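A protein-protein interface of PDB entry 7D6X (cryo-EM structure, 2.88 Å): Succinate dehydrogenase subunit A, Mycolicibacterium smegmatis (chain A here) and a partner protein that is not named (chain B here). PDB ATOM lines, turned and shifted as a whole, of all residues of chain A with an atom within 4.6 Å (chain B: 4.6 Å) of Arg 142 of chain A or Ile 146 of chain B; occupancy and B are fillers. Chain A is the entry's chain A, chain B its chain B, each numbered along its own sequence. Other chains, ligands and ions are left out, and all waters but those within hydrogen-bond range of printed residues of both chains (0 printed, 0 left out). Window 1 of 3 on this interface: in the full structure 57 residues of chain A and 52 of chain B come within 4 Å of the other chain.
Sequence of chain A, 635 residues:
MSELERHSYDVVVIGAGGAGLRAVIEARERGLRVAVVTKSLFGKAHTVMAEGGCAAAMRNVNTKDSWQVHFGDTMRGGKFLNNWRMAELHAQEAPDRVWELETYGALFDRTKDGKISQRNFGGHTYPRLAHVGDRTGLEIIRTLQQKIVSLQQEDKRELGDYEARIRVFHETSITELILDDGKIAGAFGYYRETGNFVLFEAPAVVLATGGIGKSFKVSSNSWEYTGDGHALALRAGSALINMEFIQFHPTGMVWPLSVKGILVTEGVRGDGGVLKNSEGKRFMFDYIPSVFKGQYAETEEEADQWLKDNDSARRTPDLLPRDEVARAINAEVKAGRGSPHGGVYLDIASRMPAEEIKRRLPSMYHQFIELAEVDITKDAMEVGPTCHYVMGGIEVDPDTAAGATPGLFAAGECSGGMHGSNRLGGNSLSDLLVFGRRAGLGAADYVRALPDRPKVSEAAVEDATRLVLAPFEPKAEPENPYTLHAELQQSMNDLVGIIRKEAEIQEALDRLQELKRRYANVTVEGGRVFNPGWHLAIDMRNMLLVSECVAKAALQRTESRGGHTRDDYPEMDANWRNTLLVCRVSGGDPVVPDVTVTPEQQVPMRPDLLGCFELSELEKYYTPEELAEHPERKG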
ATOM      1  N   GLY A  43      11.188  26.096  -9.755  1.00  0.00           N
ATOM      2  CA  GLY A  43      12.513  25.517  -9.753  1.00  0.00           C
ATOM      3  C   GLY A  43      13.365  25.841  -8.550  1.00  0.00           C
ATOM      4  O   GLY A  43      14.578  25.624  -8.597  1.00  0.00           O
ATOM      5  N   LYS A  44      12.774  26.353  -7.473  1.00  0.00           N
ATOM      6  CA  LYS A  44      13.506  26.686  -6.260  1.00  0.00           C
ATOM      7  C   LYS A  44      13.038  25.851  -5.076  1.00  0.00           C
ATOM      8  O   LYS A  44      13.054  26.310  -3.935  1.00  0.00           O
ATOM      9  CB  LYS A  44      13.377  28.175  -5.955  1.00  0.00           C
ATOM     10  CG  LYS A  44      13.676  29.042  -7.151  1.00  0.00           C
ATOM     11  CD  LYS A  44      14.157  30.403  -6.754  1.00  0.00           C
ATOM     12  CE  LYS A  44      14.601  31.172  -7.968  1.00  0.00           C
ATOM     13  NZ  LYS A  44      15.469  30.339  -8.821  1.00  0.00           N
ATOM     14  N   LEU A 138      20.050  19.768  -7.908  1.00  0.00           N
ATOM     15  CA  LEU A 138      19.970  20.906  -8.816  1.00  0.00           C
ATOM     16  C   LEU A 138      19.849  20.444 -10.257  1.00  0.00           C
ATOM     17  O   LEU A 138      19.026  20.964 -11.016  1.00  0.00           O
ATOM     18  CB  LEU A 138      21.191  21.805  -8.644  1.00  0.00           C
ATOM     19  CG  LEU A 138      21.314  22.962  -9.633  1.00  0.00           C
ATOM     20  CD1 LEU A 138      20.160  23.915  -9.470  1.00  0.00           C
ATOM     21  CD2 LEU A 138      22.622  23.682  -9.434  1.00  0.00           C
ATOM     22  N   GLU A 139      20.658  19.460 -10.650  1.00  0.00           N
ATOM     23  CA  GLU A 139      20.567  18.922 -12.002  1.00  0.00           C
ATOM     24  C   GLU A 139      19.201  18.306 -12.259  1.00  0.00           C
ATOM     25  O   GLU A 139      18.602  18.529 -13.315  1.00  0.00           O
ATOM     26  CB  GLU A 139      21.669  17.891 -12.226  1.00  0.00           C
ATOM     27  CG  GLU A 139      21.673  17.265 -13.607  1.00  0.00           C
ATOM     28  CD  GLU A 139      22.239  18.189 -14.668  1.00  0.00           C
ATOM     29  OE1 GLU A 139      21.644  18.276 -15.759  1.00  0.00           O
ATOM     30  OE2 GLU A 139      23.280  18.829 -14.413  1.00  0.00           O
ATOM     31  N   ILE A 140      18.685  17.543 -11.297  1.00  0.00           N
ATOM     32  CA  ILE A 140      17.394  16.886 -11.486  1.00  0.00           C
ATOM     33  C   ILE A 140      16.286  17.916 -11.652  1.00  0.00           C
ATOM     34  O   ILE A 140      15.440  17.810 -12.549  1.00  0.00           O
ATOM     35  CB  ILE A 140      17.100  15.940 -10.311  1.00  0.00           C
ATOM     36  CG1 ILE A 140      18.063  14.762 -10.328  1.00  0.00           C
ATOM     37  CG2 ILE A 140      15.675  15.447 -10.371  1.00  0.00           C
ATOM     38  CD1 ILE A 140      18.032  13.979  -9.066  1.00  0.00           C
ATOM     39  N   ILE A 141      16.274  18.932 -10.792  1.00  0.00           N
ATOM     40  CA  ILE A 141      15.177  19.888 -10.815  1.00  0.00           C
ATOM     41  C   ILE A 141      15.283  20.803 -12.030  1.00  0.00           C
ATOM     42  O   ILE A 141      14.266  21.182 -12.621  1.00  0.00           O
ATOM     43  CB  ILE A 141      15.127  20.666  -9.489  1.00  0.00           C
ATOM     44  CG1 ILE A 141      13.739  21.256  -9.270  1.00  0.00           C
ATOM     45  CG2 ILE A 141      16.171  21.750  -9.451  1.00  0.00           C
ATOM     46  CD1 ILE A 141      13.505  21.707  -7.863  1.00  0.00           C
ATOM     47  N   ARG A 142      16.506  21.136 -12.458  1.00  0.00           N
ATOM     48  CA  ARG A 142      16.662  21.878 -13.703  1.00  0.00           C
ATOM     49  C   ARG A 142      16.159  21.067 -14.881  1.00  0.00           C
ATOM     50  O   ARG A 142      15.466  21.595 -15.755  1.00  0.00           O
ATOM     51  CB  ARG A 142      18.121  22.252 -13.928  1.00  0.00           C
ATOM     52  CG  ARG A 142      18.548  23.534 -13.282  1.00  0.00           C
ATOM     53  CD  ARG A 142      17.709  24.711 -13.716  1.00  0.00           C
ATOM     54  NE  ARG A 142      17.975  25.849 -12.850  1.00  0.00           N
ATOM     55  CZ  ARG A 142      17.414  26.020 -11.661  1.00  0.00           C
ATOM     56  NH1 ARG A 142      16.544  25.137 -11.205  1.00  0.00           N
ATOM     57  NH2 ARG A 142      17.715  27.075 -10.929  1.00  0.00           N
ATOM     58  N   THR A 143      16.514  19.785 -14.928  1.00  0.00           N
ATOM     59  CA  THR A 143      16.082  18.935 -16.027  1.00  0.00           C
ATOM     60  C   THR A 143      14.565  18.860 -16.091  1.00  0.00           C
ATOM     61  O   THR A 143      13.972  18.997 -17.165  1.00  0.00           O
ATOM     62  CB  THR A 143      16.684  17.548 -15.864  1.00  0.00           C
ATOM     63  OG1 THR A 143      18.038  17.675 -15.421  1.00  0.00           O
ATOM     64  CG2 THR A 143      16.672  16.821 -17.168  1.00  0.00           C
ATOM     65  N   LEU A 144      13.918  18.669 -14.943  1.00  0.00           N
ATOM     66  CA  LEU A 144      12.466  18.543 -14.941  1.00  0.00           C
ATOM     67  C   LEU A 144      11.788  19.859 -15.304  1.00  0.00           C
ATOM     68  O   LEU A 144      10.806  19.871 -16.054  1.00  0.00           O
ATOM     69  CB  LEU A 144      11.990  18.041 -13.584  1.00  0.00           C
ATOM     70  CG  LEU A 144      12.415  16.614 -13.254  1.00  0.00           C
ATOM     71  CD1 LEU A 144      11.944  16.226 -11.875  1.00  0.00           C
ATOM     72  CD2 LEU A 144      11.878  15.654 -14.288  1.00  0.00           C
ATOM     73  N   GLN A 145      12.300  20.981 -14.796  1.00  0.00           N
ATOM     74  CA  GLN A 145      11.708  22.274 -15.124  1.00  0.00           C
ATOM     75  C   GLN A 145      11.851  22.588 -16.608  1.00  0.00           C
ATOM     76  O   GLN A 145      10.895  23.033 -17.258  1.00  0.00           O
ATOM     77  CB  GLN A 145      12.357  23.357 -14.269  1.00  0.00           C
ATOM     78  CG  GLN A 145      12.353  24.730 -14.880  1.00  0.00           C
ATOM     79  CD  GLN A 145      13.176  25.703 -14.080  1.00  0.00           C
ATOM     80  OE1 GLN A 145      13.741  25.350 -13.054  1.00  0.00           O
ATOM     81  NE2 GLN A 145      13.248  26.937 -14.546  1.00  0.00           N
ATOM     82  N   GLN A 146      13.033  22.349 -17.170  1.00  0.00           N
ATOM     83  CA  GLN A 146      13.235  22.625 -18.584  1.00  0.00           C
ATOM     84  C   GLN A 146      12.476  21.641 -19.462  1.00  0.00           C
ATOM     85  O   GLN A 146      12.085  21.989 -20.579  1.00  0.00           O
ATOM     86  CB  GLN A 146      14.725  22.618 -18.895  1.00  0.00           C
ATOM     87  CG  GLN A 146      15.475  23.713 -18.169  1.00  0.00           C
ATOM     88  CD  GLN A 146      16.964  23.502 -18.168  1.00  0.00           C
ATOM     89  OE1 GLN A 146      17.447  22.416 -18.475  1.00  0.00           O
ATOM     90  NE2 GLN A 146      17.706  24.542 -17.820  1.00  0.00           N
ATOM     91  N   GLY B  57      22.806  29.344  -0.051  1.00  0.00           N
ATOM     92  CA  GLY B  57      23.001  29.481  -1.476  1.00  0.00           C
ATOM     93  C   GLY B  57      22.976  28.402  -2.536  1.00  0.00           C
ATOM     94  O   GLY B  57      23.962  28.234  -3.254  1.00  0.00           O
ATOM     95  N   LYS B  58      21.884  27.651  -2.632  1.00  0.00           N
ATOM     96  CA  LYS B  58      21.607  26.806  -3.793  1.00  0.00           C
ATOM     97  C   LYS B  58      20.233  27.163  -4.343  1.00  0.00           C
ATOM     98  O   LYS B  58      19.577  26.323  -4.957  1.00  0.00           O
ATOM     99  CB  LYS B  58      21.463  25.717  -2.733  1.00  0.00           C
ATOM    100  CG  LYS B  58      22.782  25.113  -2.340  1.00  0.00           C
ATOM    101  CD  LYS B  58      22.645  24.194  -1.163  1.00  0.00           C
ATOM    102  CE  LYS B  58      23.911  23.395  -0.992  1.00  0.00           C
ATOM    103  NZ  LYS B  58      25.106  24.258  -1.172  1.00  0.00           N
ATOM    104  N   CYS B  59      19.768  28.370  -4.314  1.00  0.00           N
ATOM    105  CA  CYS B  59      18.529  28.843  -4.910  1.00  0.00           C
ATOM    106  C   CYS B  59      18.205  29.985  -5.856  1.00  0.00           C
ATOM    107  O   CYS B  59      17.621  29.776  -6.923  1.00  0.00           O
ATOM    108  CB  CYS B  59      17.295  28.395  -4.117  1.00  0.00           C
ATOM    109  SG  CYS B  59      16.944  29.361  -2.630  1.00  0.00           S
ATOM    110  N   GLY B  60      18.594  31.222  -5.295  1.00  0.00           N
ATOM    111  CA  GLY B  60      18.237  32.372  -6.090  1.00  0.00           C
ATOM    112  C   GLY B  60      17.056  33.140  -5.552  1.00  0.00           C
ATOM    113  O   GLY B  60      16.565  34.067  -6.199  1.00  0.00           O
ATOM    114  N   LEU B  72      23.269  37.863  -3.015  1.00  0.00           N
ATOM    115  CA  LEU B  72      22.369  37.014  -2.251  1.00  0.00           C
ATOM    116  C   LEU B  72      22.410  37.419  -0.789  1.00  0.00           C
ATOM    117  O   LEU B  72      23.481  37.621  -0.217  1.00  0.00           O
ATOM    118  CB  LEU B  72      22.761  35.546  -2.383  1.00  0.00           C
ATOM    119  CG  LEU B  72      22.683  34.876  -3.748  1.00  0.00           C
ATOM    120  CD1 LEU B  72      23.093  33.433  -3.618  1.00  0.00           C
ATOM    121  CD2 LEU B  72      21.297  34.979  -4.318  1.00  0.00           C
ATOM    122  N   ARG B 143      25.544  24.405 -16.365  1.00  0.00           N
ATOM    123  CA  ARG B 143      24.445  23.804 -15.614  1.00  0.00           C
ATOM    124  C   ARG B 143      24.552  24.034 -14.110  1.00  0.00           C
ATOM    125  O   ARG B 143      23.758  23.442 -13.383  1.00  0.00           O
ATOM    126  CB  ARG B 143      24.363  22.307 -15.902  1.00  0.00           C
ATOM    127  CG  ARG B 143      24.112  21.959 -17.355  1.00  0.00           C
ATOM    128  CD  ARG B 143      22.644  21.986 -17.695  1.00  0.00           C
ATOM    129  NE  ARG B 143      21.916  20.888 -17.073  1.00  0.00           N
ATOM    130  CZ  ARG B 143      20.614  20.679 -17.219  1.00  0.00           C
ATOM    131  NH1 ARG B 143      19.886  21.487 -17.970  1.00  0.00           N
ATOM    132  NH2 ARG B 143      20.037  19.656 -16.611  1.00  0.00           N
ATOM    133  N   LYS B 144      25.477  24.846 -13.599  1.00  0.00           N
ATOM    134  CA  LYS B 144      25.554  25.141 -12.174  1.00  0.00           C
ATOM    135  C   LYS B 144      24.671  26.303 -11.754  1.00  0.00           C
ATOM    136  O   LYS B 144      24.629  26.622 -10.564  1.00  0.00           O
ATOM    137  CB  LYS B 144      26.988  25.470 -11.769  1.00  0.00           C
ATOM    138  CG  LYS B 144      28.010  24.418 -12.083  1.00  0.00           C
ATOM    139  CD  LYS B 144      29.323  24.745 -11.405  1.00  0.00           C
ATOM    140  CE  LYS B 144      29.679  26.205 -11.591  1.00  0.00           C
ATOM    141  NZ  LYS B 144      30.998  26.533 -10.998  1.00  0.00           N
ATOM    142  N   CYS B 145      23.830  26.705 -12.776  1.00  0.00           N
ATOM    143  CA  CYS B 145      23.069  27.928 -12.527  1.00  0.00           C
ATOM    144  C   CYS B 145      21.849  28.037 -11.599  1.00  0.00           C
ATOM    145  O   CYS B 145      20.723  28.084 -12.096  1.00  0.00           O
ATOM    146  CB  CYS B 145      22.704  28.571 -13.873  1.00  0.00           C
ATOM    147  SG  CYS B 145      21.740  30.094 -13.738  1.00  0.00           S
ATOM    148  N   ILE B 146      22.231  28.328 -10.214  1.00  0.00           N
ATOM    149  CA  ILE B 146      21.052  28.613  -9.412  1.00  0.00           C
ATOM    150  C   ILE B 146      20.434  29.891  -9.949  1.00  0.00           C
ATOM    151  O   ILE B 146      21.118  30.908 -10.111  1.00  0.00           O
ATOM    152  CB  ILE B 146      21.417  28.734  -7.925  1.00  0.00           C
ATOM    153  CG1 ILE B 146      22.402  29.873  -7.686  1.00  0.00           C
ATOM    154  CG2 ILE B 146      22.030  27.447  -7.439  1.00  0.00           C
ATOM    155  CD1 ILE B 146      22.240  30.554  -6.366  1.00  0.00           C
ATOM    156  N   GLU B 147      19.155  29.842 -10.288  1.00  0.00           N
ATOM    157  CA  GLU B 147      18.608  30.963 -11.036  1.00  0.00           C
ATOM    158  C   GLU B 147      18.425  32.170 -10.132  1.00  0.00           C
ATOM    159  O   GLU B 147      17.310  32.479  -9.706  1.00  0.00           O
ATOM    160  CB  GLU B 147      17.298  30.568 -11.701  1.00  0.00           C
ATOM    161  CG  GLU B 147      17.499  29.790 -12.975  1.00  0.00           C
ATOM    162  CD  GLU B 147      16.200  29.286 -13.543  1.00  0.00           C
ATOM    163  OE1 GLU B 147      15.232  29.147 -12.769  1.00  0.00           O
ATOM    164  OE2 GLU B 147      16.141  29.028 -14.762  1.00  0.00           O
ATOM    165  N   CYS B 148      19.519  32.868  -9.848  1.00  0.00           N
ATOM    166  CA  CYS B 148      19.470  34.048  -8.990  1.00  0.00           C
ATOM    167  C   CYS B 148      19.006  35.288  -9.751  1.00  0.00           C
ATOM    168  O   CYS B 148      18.375  36.179  -9.182  1.00  0.00           O
ATOM    169  CB  CYS B 148      20.839  34.305  -8.355  1.00  0.00           C
ATOM    170  SG  CYS B 148      21.846  35.531  -9.222  1.00  0.00           S
ATOM    171  N   GLU B 215      27.723  31.632  -8.251  1.00  0.00           N
ATOM    172  CA  GLU B 215      28.331  30.362  -8.608  1.00  0.00           C
ATOM    173  C   GLU B 215      29.683  30.522  -9.276  1.00  0.00           C
ATOM    174  O   GLU B 215      30.327  29.514  -9.575  1.00  0.00           O
ATOM    175  CB  GLU B 215      27.399  29.581  -9.528  1.00  0.00           C
ATOM    176  CG  GLU B 215      26.038  29.341  -8.939  1.00  0.00           C
ATOM    177  CD  GLU B 215      26.083  28.390  -7.769  1.00  0.00           C
ATOM    178  OE1 GLU B 215      26.222  28.860  -6.621  1.00  0.00           O
ATOM    179  OE2 GLU B 215      25.987  27.168  -7.995  1.00  0.00           O
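The side-chain amino group (NZ) of Lys 44 of chain A lies within hydrogen-bond range of the backbone carbonyl oxygen (O) of Glu 147 of chain B (3.0 Å). O of Cys 145 of chain B is in hydrogen-bond range of NH2 of Arg 142 of chain A. The side-chain amide oxygen of Gln 146 of chain A sits at hydrogen-bond distance from the guanidinium group of Arg 143 of chain B (2.7 Å). OG1 of Thr 143 of chain A sits at hydrogen-bond distance from NH2 of Arg 143 of chain B (3.1 Å). O of Cys 59 of chain B is in hydrogen-bond range of NZ of Lys 44 of chain A (2.9 Å). OE1 of Glu 139 of chain A is in salt-bridge range of NE of Arg 143 of chain B, 2.9 Å away. The guanidinium group (NH2) of Arg 142 of chain A is in salt-bridge range of the side-chain carboxylate (OE1) of Glu 147 of chain B, 3.7 Å away. The side-chain amide nitrogen (NE2) of Gln 145 of chain A is in hydrogen-bond range of the side-chain carboxylate (OE1) of Glu 147 of chain B.
Among the printed residues, pairs that only touch across the chains: Leu 138 of chain A with Lys 144 of chain B, Lys 44 of chain A with Gly 60 of chain B and Arg 142 of chain A with Ile 146 of chain B.
The side-chain amino group (NZ) of Lys 144 of chain B sits at hydrogen-bond distance from the backbone carbonyl oxygen (O) of Glu 215 of chain B (3.4 Å). The side-chain amide oxygen (OE1) of Gln 146 of chain A lies close to the backbone carbonyl oxygen (O) of Arg 142 of chain A (3.5 Å). O of Gly 43 of chain A is in hydrogen-bond range of NH1 of Arg 142 of chain A (3.3 Å). NH1 of Arg 142 of chain A is in hydrogen-bond range of OE1 of Gln 145 of chain A, 3.4 Å away.
Of the 11 printed residues of chain A, 7 touch a printed residue of chain B. Printed residues of chain A that touch a printed residue of chain B: Lys 44, Leu 138, Glu 139, Arg 142, Thr 143, Gln 145 and Gln 146. Along chain A the printed residues that touch a printed residue of chain B span positions 44 to 146. Among the printed residues, 11 pairs touch across the chains. Among the printed residues, Asp or Glu carboxylates within 4 Å of a Lys or Arg side-chain nitrogen of the other chain: Glu 139 of chain A with Arg 143 of chain B (2.3 Å) and Arg 142 of chain A with Glu 147 of chain B (3.7 Å).
Of the printed residues of chain B, Lys 44 of chain A touches Cys 59, Gly 60 and Glu 147. Ile 140 of chain A touches none of the printed residues of chain B. Arg 142 of chain A touches just these residues of chain B: Cys 145, Ile 146 and Glu 147. Gly 57 of chain B touches none of the printed residues of chain A. Printed residues of chain A within 4 Å of Cys 145 of chain B: Arg 142 (3.4 Å). Of chain A, only Arg 142 (3.98 Å) comes within 4 Å of Ile 146 of chain B. Printed residues of chain A within 4 Å of Glu 147 of chain B: Lys 44 (3.0 Å), Arg 142 (3.2 Å) and Gln 145 (3.5 Å). The nearest printed residue of chain A that does not touch Lys 144 of chain B is Glu 139 of chain A (6.5 Å).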
